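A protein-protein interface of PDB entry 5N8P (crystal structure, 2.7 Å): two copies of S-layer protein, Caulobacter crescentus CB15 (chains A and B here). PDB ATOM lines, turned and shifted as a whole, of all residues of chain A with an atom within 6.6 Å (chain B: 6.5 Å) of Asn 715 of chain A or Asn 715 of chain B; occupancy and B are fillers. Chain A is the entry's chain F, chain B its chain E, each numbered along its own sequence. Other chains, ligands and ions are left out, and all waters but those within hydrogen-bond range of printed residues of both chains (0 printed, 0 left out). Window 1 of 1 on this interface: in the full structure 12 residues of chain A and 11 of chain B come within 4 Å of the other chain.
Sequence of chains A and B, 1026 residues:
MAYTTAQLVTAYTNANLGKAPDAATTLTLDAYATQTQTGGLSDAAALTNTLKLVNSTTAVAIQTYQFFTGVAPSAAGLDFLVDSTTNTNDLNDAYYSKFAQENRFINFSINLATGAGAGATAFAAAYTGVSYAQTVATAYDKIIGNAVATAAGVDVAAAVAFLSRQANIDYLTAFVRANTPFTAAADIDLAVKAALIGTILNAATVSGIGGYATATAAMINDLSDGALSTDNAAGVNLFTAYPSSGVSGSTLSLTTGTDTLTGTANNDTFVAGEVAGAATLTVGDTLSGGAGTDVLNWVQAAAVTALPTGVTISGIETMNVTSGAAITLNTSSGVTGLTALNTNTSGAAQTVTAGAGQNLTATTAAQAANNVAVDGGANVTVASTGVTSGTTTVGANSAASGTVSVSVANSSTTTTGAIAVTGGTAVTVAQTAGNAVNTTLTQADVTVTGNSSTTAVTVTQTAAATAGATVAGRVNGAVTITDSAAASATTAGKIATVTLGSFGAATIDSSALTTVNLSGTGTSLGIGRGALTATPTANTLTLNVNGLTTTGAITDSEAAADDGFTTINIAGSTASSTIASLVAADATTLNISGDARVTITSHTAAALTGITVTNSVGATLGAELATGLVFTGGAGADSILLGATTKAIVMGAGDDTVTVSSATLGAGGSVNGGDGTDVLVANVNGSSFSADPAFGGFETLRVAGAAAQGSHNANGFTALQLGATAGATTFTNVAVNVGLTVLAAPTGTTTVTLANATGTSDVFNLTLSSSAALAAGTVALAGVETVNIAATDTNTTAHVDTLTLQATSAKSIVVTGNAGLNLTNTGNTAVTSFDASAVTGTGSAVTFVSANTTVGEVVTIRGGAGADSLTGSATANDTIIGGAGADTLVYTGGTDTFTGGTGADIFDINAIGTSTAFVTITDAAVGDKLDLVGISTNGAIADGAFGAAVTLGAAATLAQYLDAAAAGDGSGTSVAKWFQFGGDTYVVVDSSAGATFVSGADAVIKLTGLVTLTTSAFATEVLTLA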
ATOM      1  N   PHE A 689     -17.649 -15.327  -6.728  1.00  0.00           N
ATOM      2  CA  PHE A 689     -17.035 -14.427  -7.700  1.00  0.00           C
ATOM      3  C   PHE A 689     -17.756 -13.103  -7.862  1.00  0.00           C
ATOM      4  O   PHE A 689     -17.154 -12.093  -8.241  1.00  0.00           O
ATOM      5  CB  PHE A 689     -16.800 -15.133  -9.049  1.00  0.00           C
ATOM      6  CG  PHE A 689     -15.823 -16.275  -8.965  1.00  0.00           C
ATOM      7  CD1 PHE A 689     -16.220 -17.551  -9.270  1.00  0.00           C
ATOM      8  CD2 PHE A 689     -14.503 -16.067  -8.547  1.00  0.00           C
ATOM      9  CE1 PHE A 689     -15.318 -18.607  -9.197  1.00  0.00           C
ATOM     10  CE2 PHE A 689     -13.602 -17.114  -8.448  1.00  0.00           C
ATOM     11  CZ  PHE A 689     -14.008 -18.386  -8.783  1.00  0.00           C
ATOM     12  N   SER A 690     -19.037 -13.099  -7.540  1.00  0.00           N
ATOM     13  CA  SER A 690     -19.803 -11.897  -7.703  1.00  0.00           C
ATOM     14  C   SER A 690     -19.325 -10.782  -6.764  1.00  0.00           C
ATOM     15  O   SER A 690     -19.188  -9.618  -7.163  1.00  0.00           O
ATOM     16  CB  SER A 690     -21.255 -12.197  -7.460  1.00  0.00           C
ATOM     17  OG  SER A 690     -21.963 -11.625  -8.523  1.00  0.00           O
ATOM     18  N   ALA A 691     -19.069 -11.178  -5.520  1.00  0.00           N
ATOM     19  CA  ALA A 691     -18.539 -10.295  -4.501  1.00  0.00           C
ATOM     20  C   ALA A 691     -17.198  -9.611  -4.869  1.00  0.00           C
ATOM     21  O   ALA A 691     -17.057  -8.394  -4.672  1.00  0.00           O
ATOM     22  CB  ALA A 691     -18.386 -11.068  -3.211  1.00  0.00           C
ATOM     23  N   LEU A 701     -21.305 -19.564 -14.728  1.00  0.00           N
ATOM     24  CA  LEU A 701     -20.392 -20.145 -13.771  1.00  0.00           C
ATOM     25  C   LEU A 701     -20.417 -21.650 -13.985  1.00  0.00           C
ATOM     26  O   LEU A 701     -21.490 -22.258 -13.926  1.00  0.00           O
ATOM     27  CB  LEU A 701     -20.797 -19.769 -12.338  1.00  0.00           C
ATOM     28  CG  LEU A 701     -20.127 -20.555 -11.213  1.00  0.00           C
ATOM     29  CD1 LEU A 701     -18.706 -20.080 -10.986  1.00  0.00           C
ATOM     30  CD2 LEU A 701     -20.908 -20.459  -9.915  1.00  0.00           C
ATOM     31  N   HIS A 712     -20.672 -22.953  -3.821  1.00  0.00           N
ATOM     32  CA  HIS A 712     -20.376 -21.961  -4.871  1.00  0.00           C
ATOM     33  C   HIS A 712     -21.446 -20.898  -5.049  1.00  0.00           C
ATOM     34  O   HIS A 712     -22.566 -21.221  -5.396  1.00  0.00           O
ATOM     35  CB  HIS A 712     -20.109 -22.668  -6.219  1.00  0.00           C
ATOM     36  CG  HIS A 712     -18.790 -23.375  -6.277  1.00  0.00           C
ATOM     37  ND1 HIS A 712     -17.667 -22.798  -6.824  1.00  0.00           N
ATOM     38  CD2 HIS A 712     -18.404 -24.591  -5.820  1.00  0.00           C
ATOM     39  CE1 HIS A 712     -16.648 -23.630  -6.705  1.00  0.00           C
ATOM     40  NE2 HIS A 712     -17.067 -24.728  -6.108  1.00  0.00           N
ATOM     41  N   ASN A 713     -21.108 -19.635  -4.841  1.00  0.00           N
ATOM     42  CA  ASN A 713     -22.128 -18.578  -4.945  1.00  0.00           C
ATOM     43  C   ASN A 713     -22.516 -18.227  -6.383  1.00  0.00           C
ATOM     44  O   ASN A 713     -21.796 -17.500  -7.082  1.00  0.00           O
ATOM     45  CB  ASN A 713     -21.784 -17.313  -4.104  1.00  0.00           C
ATOM     46  CG  ASN A 713     -22.893 -16.241  -4.157  1.00  0.00           C
ATOM     47  OD1 ASN A 713     -24.049 -16.520  -4.478  1.00  0.00           O
ATOM     48  ND2 ASN A 713     -22.527 -15.000  -3.854  1.00  0.00           N
ATOM     49  N   ALA A 714     -23.693 -18.720  -6.766  1.00  0.00           N
ATOM     50  CA  ALA A 714     -24.309 -18.487  -8.079  1.00  0.00           C
ATOM     51  C   ALA A 714     -24.736 -17.057  -8.345  1.00  0.00           C
ATOM     52  O   ALA A 714     -25.026 -16.703  -9.491  1.00  0.00           O
ATOM     53  CB  ALA A 714     -25.499 -19.421  -8.286  1.00  0.00           C
ATOM     54  N   ASN A 715     -24.767 -16.239  -7.297  1.00  0.00           N
ATOM     55  CA  ASN A 715     -25.304 -14.886  -7.415  1.00  0.00           C
ATOM     56  C   ASN A 715     -24.603 -14.138  -8.519  1.00  0.00           C
ATOM     57  O   ASN A 715     -23.364 -14.222  -8.661  1.00  0.00           O
ATOM     58  CB  ASN A 715     -25.230 -14.084  -6.102  1.00  0.00           C
ATOM     59  CG  ASN A 715     -25.885 -12.724  -6.205  1.00  0.00           C
ATOM     60  OD1 ASN A 715     -25.245 -11.702  -5.890  1.00  0.00           O
ATOM     61  ND2 ASN A 715     -27.142 -12.693  -6.693  1.00  0.00           N
ATOM     62  N   GLY A 716     -25.444 -13.455  -9.300  1.00  0.00           N
ATOM     63  CA  GLY A 716     -25.036 -12.571 -10.378  1.00  0.00           C
ATOM     64  C   GLY A 716     -24.619 -13.262 -11.666  1.00  0.00           C
ATOM     65  O   GLY A 716     -24.163 -12.598 -12.580  1.00  0.00           O
ATOM     66  N   PHE A 717     -24.743 -14.592 -11.725  1.00  0.00           N
ATOM     67  CA  PHE A 717     -24.589 -15.343 -12.987  1.00  0.00           C
ATOM     68  C   PHE A 717     -25.947 -15.577 -13.636  1.00  0.00           C
ATOM     69  O   PHE A 717     -26.949 -15.758 -12.935  1.00  0.00           O
ATOM     70  CB  PHE A 717     -23.854 -16.675 -12.755  1.00  0.00           C
ATOM     71  CG  PHE A 717     -22.414 -16.510 -12.298  1.00  0.00           C
ATOM     72  CD1 PHE A 717     -21.397 -16.207 -13.207  1.00  0.00           C
ATOM     73  CD2 PHE A 717     -22.077 -16.665 -10.950  1.00  0.00           C
ATOM     74  CE1 PHE A 717     -20.078 -16.051 -12.786  1.00  0.00           C
ATOM     75  CE2 PHE A 717     -20.751 -16.524 -10.517  1.00  0.00           C
ATOM     76  CZ  PHE A 717     -19.750 -16.217 -11.446  1.00  0.00           C
ATOM     77  N   THR A 732     -25.403 -22.106  -4.458  1.00  0.00           N
ATOM     78  CA  THR A 732     -26.245 -21.292  -3.552  1.00  0.00           C
ATOM     79  C   THR A 732     -26.696 -20.000  -4.238  1.00  0.00           C
ATOM     80  O   THR A 732     -26.067 -19.573  -5.200  1.00  0.00           O
ATOM     81  CB  THR A 732     -25.503 -20.915  -2.233  1.00  0.00           C
ATOM     82  OG1 THR A 732     -24.320 -20.188  -2.546  1.00  0.00           O
ATOM     83  CG2 THR A 732     -25.123 -22.154  -1.384  1.00  0.00           C
ATOM     84  N   ASN A 733     -27.761 -19.385  -3.734  1.00  0.00           N
ATOM     85  CA  ASN A 733     -28.213 -18.045  -4.183  1.00  0.00           C
ATOM     86  C   ASN A 733     -28.544 -17.970  -5.672  1.00  0.00           C
ATOM     87  O   ASN A 733     -28.371 -16.920  -6.310  1.00  0.00           O
ATOM     88  CB  ASN A 733     -27.220 -16.925  -3.767  1.00  0.00           C
ATOM     89  CG  ASN A 733     -27.068 -16.795  -2.266  1.00  0.00           C
ATOM     90  OD1 ASN A 733     -28.052 -16.601  -1.534  1.00  0.00           O
ATOM     91  ND2 ASN A 733     -25.835 -16.902  -1.792  1.00  0.00           N
ATOM     92  N   VAL A 734     -29.045 -19.092  -6.193  1.00  0.00           N
ATOM     93  CA  VAL A 734     -29.401 -19.243  -7.604  1.00  0.00           C
ATOM     94  C   VAL A 734     -30.659 -18.431  -7.912  1.00  0.00           C
ATOM     95  O   VAL A 734     -31.735 -18.743  -7.402  1.00  0.00           O
ATOM     96  CB  VAL A 734     -29.655 -20.717  -7.971  1.00  0.00           C
ATOM     97  CG1 VAL A 734     -29.963 -20.845  -9.459  1.00  0.00           C
ATOM     98  CG2 VAL A 734     -28.469 -21.586  -7.567  1.00  0.00           C
ATOM     99  N   ALA A 735     -30.502 -17.408  -8.772  1.00  0.00           N
ATOM    100  CA  ALA A 735     -31.618 -16.545  -9.183  1.00  0.00           C
ATOM    101  C   ALA A 735     -32.652 -17.297 -10.035  1.00  0.00           C
ATOM    102  O   ALA A 735     -32.379 -18.400 -10.559  1.00  0.00           O
ATOM    103  CB  ALA A 735     -31.103 -15.329  -9.922  1.00  0.00           C
ATOM    104  N   PHE B 689     -29.636 -12.224   2.399  1.00  0.00           N
ATOM    105  CA  PHE B 689     -30.819 -11.448   2.037  1.00  0.00           C
ATOM    106  C   PHE B 689     -30.767 -10.805   0.668  1.00  0.00           C
ATOM    107  O   PHE B 689     -31.803 -10.537   0.042  1.00  0.00           O
ATOM    108  CB  PHE B 689     -31.235 -10.463   3.142  1.00  0.00           C
ATOM    109  CG  PHE B 689     -31.613 -11.125   4.436  1.00  0.00           C
ATOM    110  CD1 PHE B 689     -30.867 -10.938   5.583  1.00  0.00           C
ATOM    111  CD2 PHE B 689     -32.704 -11.966   4.485  1.00  0.00           C
ATOM    112  CE1 PHE B 689     -31.228 -11.551   6.775  1.00  0.00           C
ATOM    113  CE2 PHE B 689     -33.075 -12.593   5.694  1.00  0.00           C
ATOM    114  CZ  PHE B 689     -32.315 -12.405   6.821  1.00  0.00           C
ATOM    115  N   SER B 690     -29.564 -10.592   0.187  1.00  0.00           N
ATOM    116  CA  SER B 690     -29.414  -9.944  -1.093  1.00  0.00           C
ATOM    117  C   SER B 690     -29.966 -10.799  -2.231  1.00  0.00           C
ATOM    118  O   SER B 690     -30.668 -10.295  -3.133  1.00  0.00           O
ATOM    119  CB  SER B 690     -27.970  -9.638  -1.347  1.00  0.00           C
ATOM    120  OG  SER B 690     -27.932  -8.282  -1.729  1.00  0.00           O
ATOM    121  N   ALA B 691     -29.656 -12.100  -2.157  1.00  0.00           N
ATOM    122  CA  ALA B 691     -30.153 -13.077  -3.097  1.00  0.00           C
ATOM    123  C   ALA B 691     -31.699 -13.143  -3.223  1.00  0.00           C
ATOM    124  O   ALA B 691     -32.225 -13.178  -4.344  1.00  0.00           O
ATOM    125  CB  ALA B 691     -29.601 -14.433  -2.714  1.00  0.00           C
ATOM    126  N   LEU B 701     -27.463  -4.316   7.525  1.00  0.00           N
ATOM    127  CA  LEU B 701     -27.724  -5.632   8.037  1.00  0.00           C
ATOM    128  C   LEU B 701     -27.176  -5.689   9.447  1.00  0.00           C
ATOM    129  O   LEU B 701     -25.991  -5.417   9.644  1.00  0.00           O
ATOM    130  CB  LEU B 701     -27.071  -6.700   7.139  1.00  0.00           C
ATOM    131  CG  LEU B 701     -26.979  -8.117   7.714  1.00  0.00           C
ATOM    132  CD1 LEU B 701     -28.302  -8.805   7.632  1.00  0.00           C
ATOM    133  CD2 LEU B 701     -25.957  -8.953   7.018  1.00  0.00           C
ATOM    134  N   HIS B 712     -23.117 -14.880   7.564  1.00  0.00           N
ATOM    135  CA  HIS B 712     -24.117 -13.905   7.070  1.00  0.00           C
ATOM    136  C   HIS B 712     -23.660 -13.136   5.838  1.00  0.00           C
ATOM    137  O   HIS B 712     -22.666 -12.415   5.893  1.00  0.00           O
ATOM    138  CB  HIS B 712     -24.497 -12.915   8.191  1.00  0.00           C
ATOM    139  CG  HIS B 712     -25.393 -13.513   9.234  1.00  0.00           C
ATOM    140  ND1 HIS B 712     -26.771 -13.384   9.212  1.00  0.00           N
ATOM    141  CD2 HIS B 712     -25.103 -14.275  10.315  1.00  0.00           C
ATOM    142  CE1 HIS B 712     -27.283 -14.045  10.232  1.00  0.00           C
ATOM    143  NE2 HIS B 712     -26.292 -14.589  10.919  1.00  0.00           N
ATOM    144  N   ASN B 713     -24.396 -13.250   4.737  1.00  0.00           N
ATOM    145  CA  ASN B 713     -23.958 -12.583   3.500  1.00  0.00           C
ATOM    146  C   ASN B 713     -24.207 -11.071   3.493  1.00  0.00           C
ATOM    147  O   ASN B 713     -25.342 -10.616   3.256  1.00  0.00           O
ATOM    148  CB  ASN B 713     -24.493 -13.268   2.203  1.00  0.00           C
ATOM    149  CG  ASN B 713     -23.987 -12.598   0.913  1.00  0.00           C
ATOM    150  OD1 ASN B 713     -22.968 -11.909   0.914  1.00  0.00           O
ATOM    151  ND2 ASN B 713     -24.698 -12.804  -0.188  1.00  0.00           N
ATOM    152  N   ALA B 714     -23.110 -10.334   3.689  1.00  0.00           N
ATOM    153  CA  ALA B 714     -23.094  -8.869   3.685  1.00  0.00           C
ATOM    154  C   ALA B 714     -23.392  -8.225   2.338  1.00  0.00           C
ATOM    155  O   ALA B 714     -23.664  -7.003   2.273  1.00  0.00           O
ATOM    156  CB  ALA B 714     -21.741  -8.359   4.184  1.00  0.00           C
ATOM    157  N   ASN B 715     -23.325  -9.032   1.267  1.00  0.00           N
ATOM    158  CA  ASN B 715     -23.422  -8.488  -0.071  1.00  0.00           C
ATOM    159  C   ASN B 715     -24.666  -7.658  -0.233  1.00  0.00           C
ATOM    160  O   ASN B 715     -25.756  -8.054   0.252  1.00  0.00           O
ATOM    161  CB  ASN B 715     -23.366  -9.562  -1.169  1.00  0.00           C
ATOM    162  CG  ASN B 715     -23.307  -8.959  -2.570  1.00  0.00           C
ATOM    163  OD1 ASN B 715     -24.091  -9.316  -3.440  1.00  0.00           O
ATOM    164  ND2 ASN B 715     -22.373  -8.010  -2.778  1.00  0.00           N
ATOM    165  N   GLY B 716     -24.449  -6.494  -0.863  1.00  0.00           N
ATOM    166  CA  GLY B 716     -25.477  -5.559  -1.247  1.00  0.00           C
ATOM    167  C   GLY B 716     -26.071  -4.711  -0.135  1.00  0.00           C
ATOM    168  O   GLY B 716     -26.998  -3.966  -0.366  1.00  0.00           O
ATOM    169  N   PHE B 717     -25.482  -4.799   1.066  1.00  0.00           N
ATOM    170  CA  PHE B 717     -25.745  -3.832   2.155  1.00  0.00           C
ATOM    171  C   PHE B 717     -24.698  -2.723   2.139  1.00  0.00           C
ATOM    172  O   PHE B 717     -23.547  -2.974   1.781  1.00  0.00           O
ATOM    173  CB  PHE B 717     -25.767  -4.545   3.509  1.00  0.00           C
ATOM    174  CG  PHE B 717     -26.906  -5.519   3.684  1.00  0.00           C
ATOM    175  CD1 PHE B 717     -28.203  -5.059   3.996  1.00  0.00           C
ATOM    176  CD2 PHE B 717     -26.692  -6.907   3.533  1.00  0.00           C
ATOM    177  CE1 PHE B 717     -29.266  -5.957   4.115  1.00  0.00           C
ATOM    178  CE2 PHE B 717     -27.756  -7.803   3.658  1.00  0.00           C
ATOM    179  CZ  PHE B 717     -29.036  -7.323   3.954  1.00  0.00           C
ATOM    180  N   THR B 732     -19.565 -12.294   5.543  1.00  0.00           N
ATOM    181  CA  THR B 732     -18.870 -12.668   4.288  1.00  0.00           C
ATOM    182  C   THR B 732     -19.218 -11.669   3.180  1.00  0.00           C
ATOM    183  O   THR B 732     -20.238 -10.969   3.261  1.00  0.00           O
ATOM    184  CB  THR B 732     -19.270 -14.094   3.806  1.00  0.00           C
ATOM    185  OG1 THR B 732     -20.690 -14.161   3.603  1.00  0.00           O
ATOM    186  CG2 THR B 732     -18.833 -15.202   4.799  1.00  0.00           C
ATOM    187  N   ASN B 733     -18.374 -11.627   2.140  1.00  0.00           N
ATOM    188  CA  ASN B 733     -18.650 -10.861   0.909  1.00  0.00           C
ATOM    189  C   ASN B 733     -18.859  -9.364   1.151  1.00  0.00           C
ATOM    190  O   ASN B 733     -19.621  -8.705   0.415  1.00  0.00           O
ATOM    191  CB  ASN B 733     -19.833 -11.467   0.099  1.00  0.00           C
ATOM    192  CG  ASN B 733     -19.583 -12.887  -0.370  1.00  0.00           C
ATOM    193  OD1 ASN B 733     -18.601 -13.186  -1.046  1.00  0.00           O
ATOM    194  ND2 ASN B 733     -20.478 -13.759  -0.042  1.00  0.00           N
ATOM    195  N   VAL B 734     -18.162  -8.845   2.163  1.00  0.00           N
ATOM    196  CA  VAL B 734     -18.240  -7.450   2.578  1.00  0.00           C
ATOM    197  C   VAL B 734     -17.590  -6.544   1.550  1.00  0.00           C
ATOM    198  O   VAL B 734     -16.373  -6.607   1.371  1.00  0.00           O
ATOM    199  CB  VAL B 734     -17.569  -7.221   3.953  1.00  0.00           C
ATOM    200  CG1 VAL B 734     -17.811  -5.776   4.400  1.00  0.00           C
ATOM    201  CG2 VAL B 734     -18.099  -8.189   4.999  1.00  0.00           C
ATOM    202  N   ALA B 735     -18.409  -5.694   0.904  1.00  0.00           N
ATOM    203  CA  ALA B 735     -17.921  -4.713  -0.077  1.00  0.00           C
ATOM    204  C   ALA B 735     -17.046  -3.631   0.569  1.00  0.00           C
ATOM    205  O   ALA B 735     -17.048  -3.441   1.790  1.00  0.00           O
ATOM    206  CB  ALA B 735     -19.096  -4.066  -0.804  1.00  0.00           C
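Phe 689 of chain A touches none of the printed residues of chain B. Of the printed residues of chain B, Ala 691 of chain A touches Asn 733 (3.0 Å). Of chain B, only Asn 715 comes within 4 Å of Asn 715 of chain A. Of the printed residues of chain B, Asn 733 of chain A touches Ala 691 (2.9 Å). Ser 690 of chain B touches none of the printed residues of chain A. Of the printed residues of chain A, Ala 691 of chain B touches Asn 733 (2.9 Å). Of chain A, only Asn 715 (3.6 Å) comes within 4 Å of Asn 715 of chain B. The nearest residue of chain B that does not touch Asn 715 of chain A is Ala 691 of chain B (4.7 Å). The nearest printed residue of chain B that does not touch Ala 691 of chain A is Asn 715 of chain B (4.8 Å).
Among the printed residues, pairs that only touch across the chains: Asn 733 of chain A with Ala 691 of chain B (2.9 Å), Ala 691 of chain A with Asn 733 of chain B (3.0 Å) and Asn 715 of chain A with Asn 715 of chain B (3.6 Å).
Printed residues of chain A that touch a printed residue of chain B: Ala 691, Asn 715 and Asn 733. Hydrophobic or aromatic side chains of chain A that line the printed part of chain B: Ala 691. Of the 14 printed residues of chain B, 3 touch a printed residue of chain A.
The backbone carbonyl oxygen (O) of Asn 715 of chain B sits at hydrogen-bond distance from the side-chain hydroxyl (OG) of Ser 690 of chain B (3.0 Å). The side-chain amide oxygen (OD1) of Asn 713 of chain B sits at hydrogen-bond distance from the backbone NH (N) of Asn 715 of chain B (2.9 Å). The side-chain amide oxygen (OD1) of Asn 713 of chain B is in hydrogen-bond range of the side-chain amide nitrogen (ND2) of Asn 733 of chain B (3.2 Å). OG of Ser 690 of chain A sits at hydrogen-bond distance from O of Asn 715 of chain A. OD1 of Asn 713 of chain A lies within hydrogen-bond range of N of Asn 715 of chain A (2.9 Å). OD1 of Asn 713 of chain A lies within hydrogen-bond range of ND2 of Asn 733 of chain A.
Ala 691 of chain A touches Asn 733 of chain B, and with the chains exchanged Asn 733 of chain A touches Ala 691 of chain B. Asn 715 of chain B touches its own counterpart, Asn 715 of chain A. Positions printed for both chains: 689, 690, 691, 701, 712, 713, 714, 715, 716, 717, 732, 733, 734 and 735. Of the 3 pairs that touch across the chains among the printed residues, 3 have their exchanged pair printed and touching as well.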
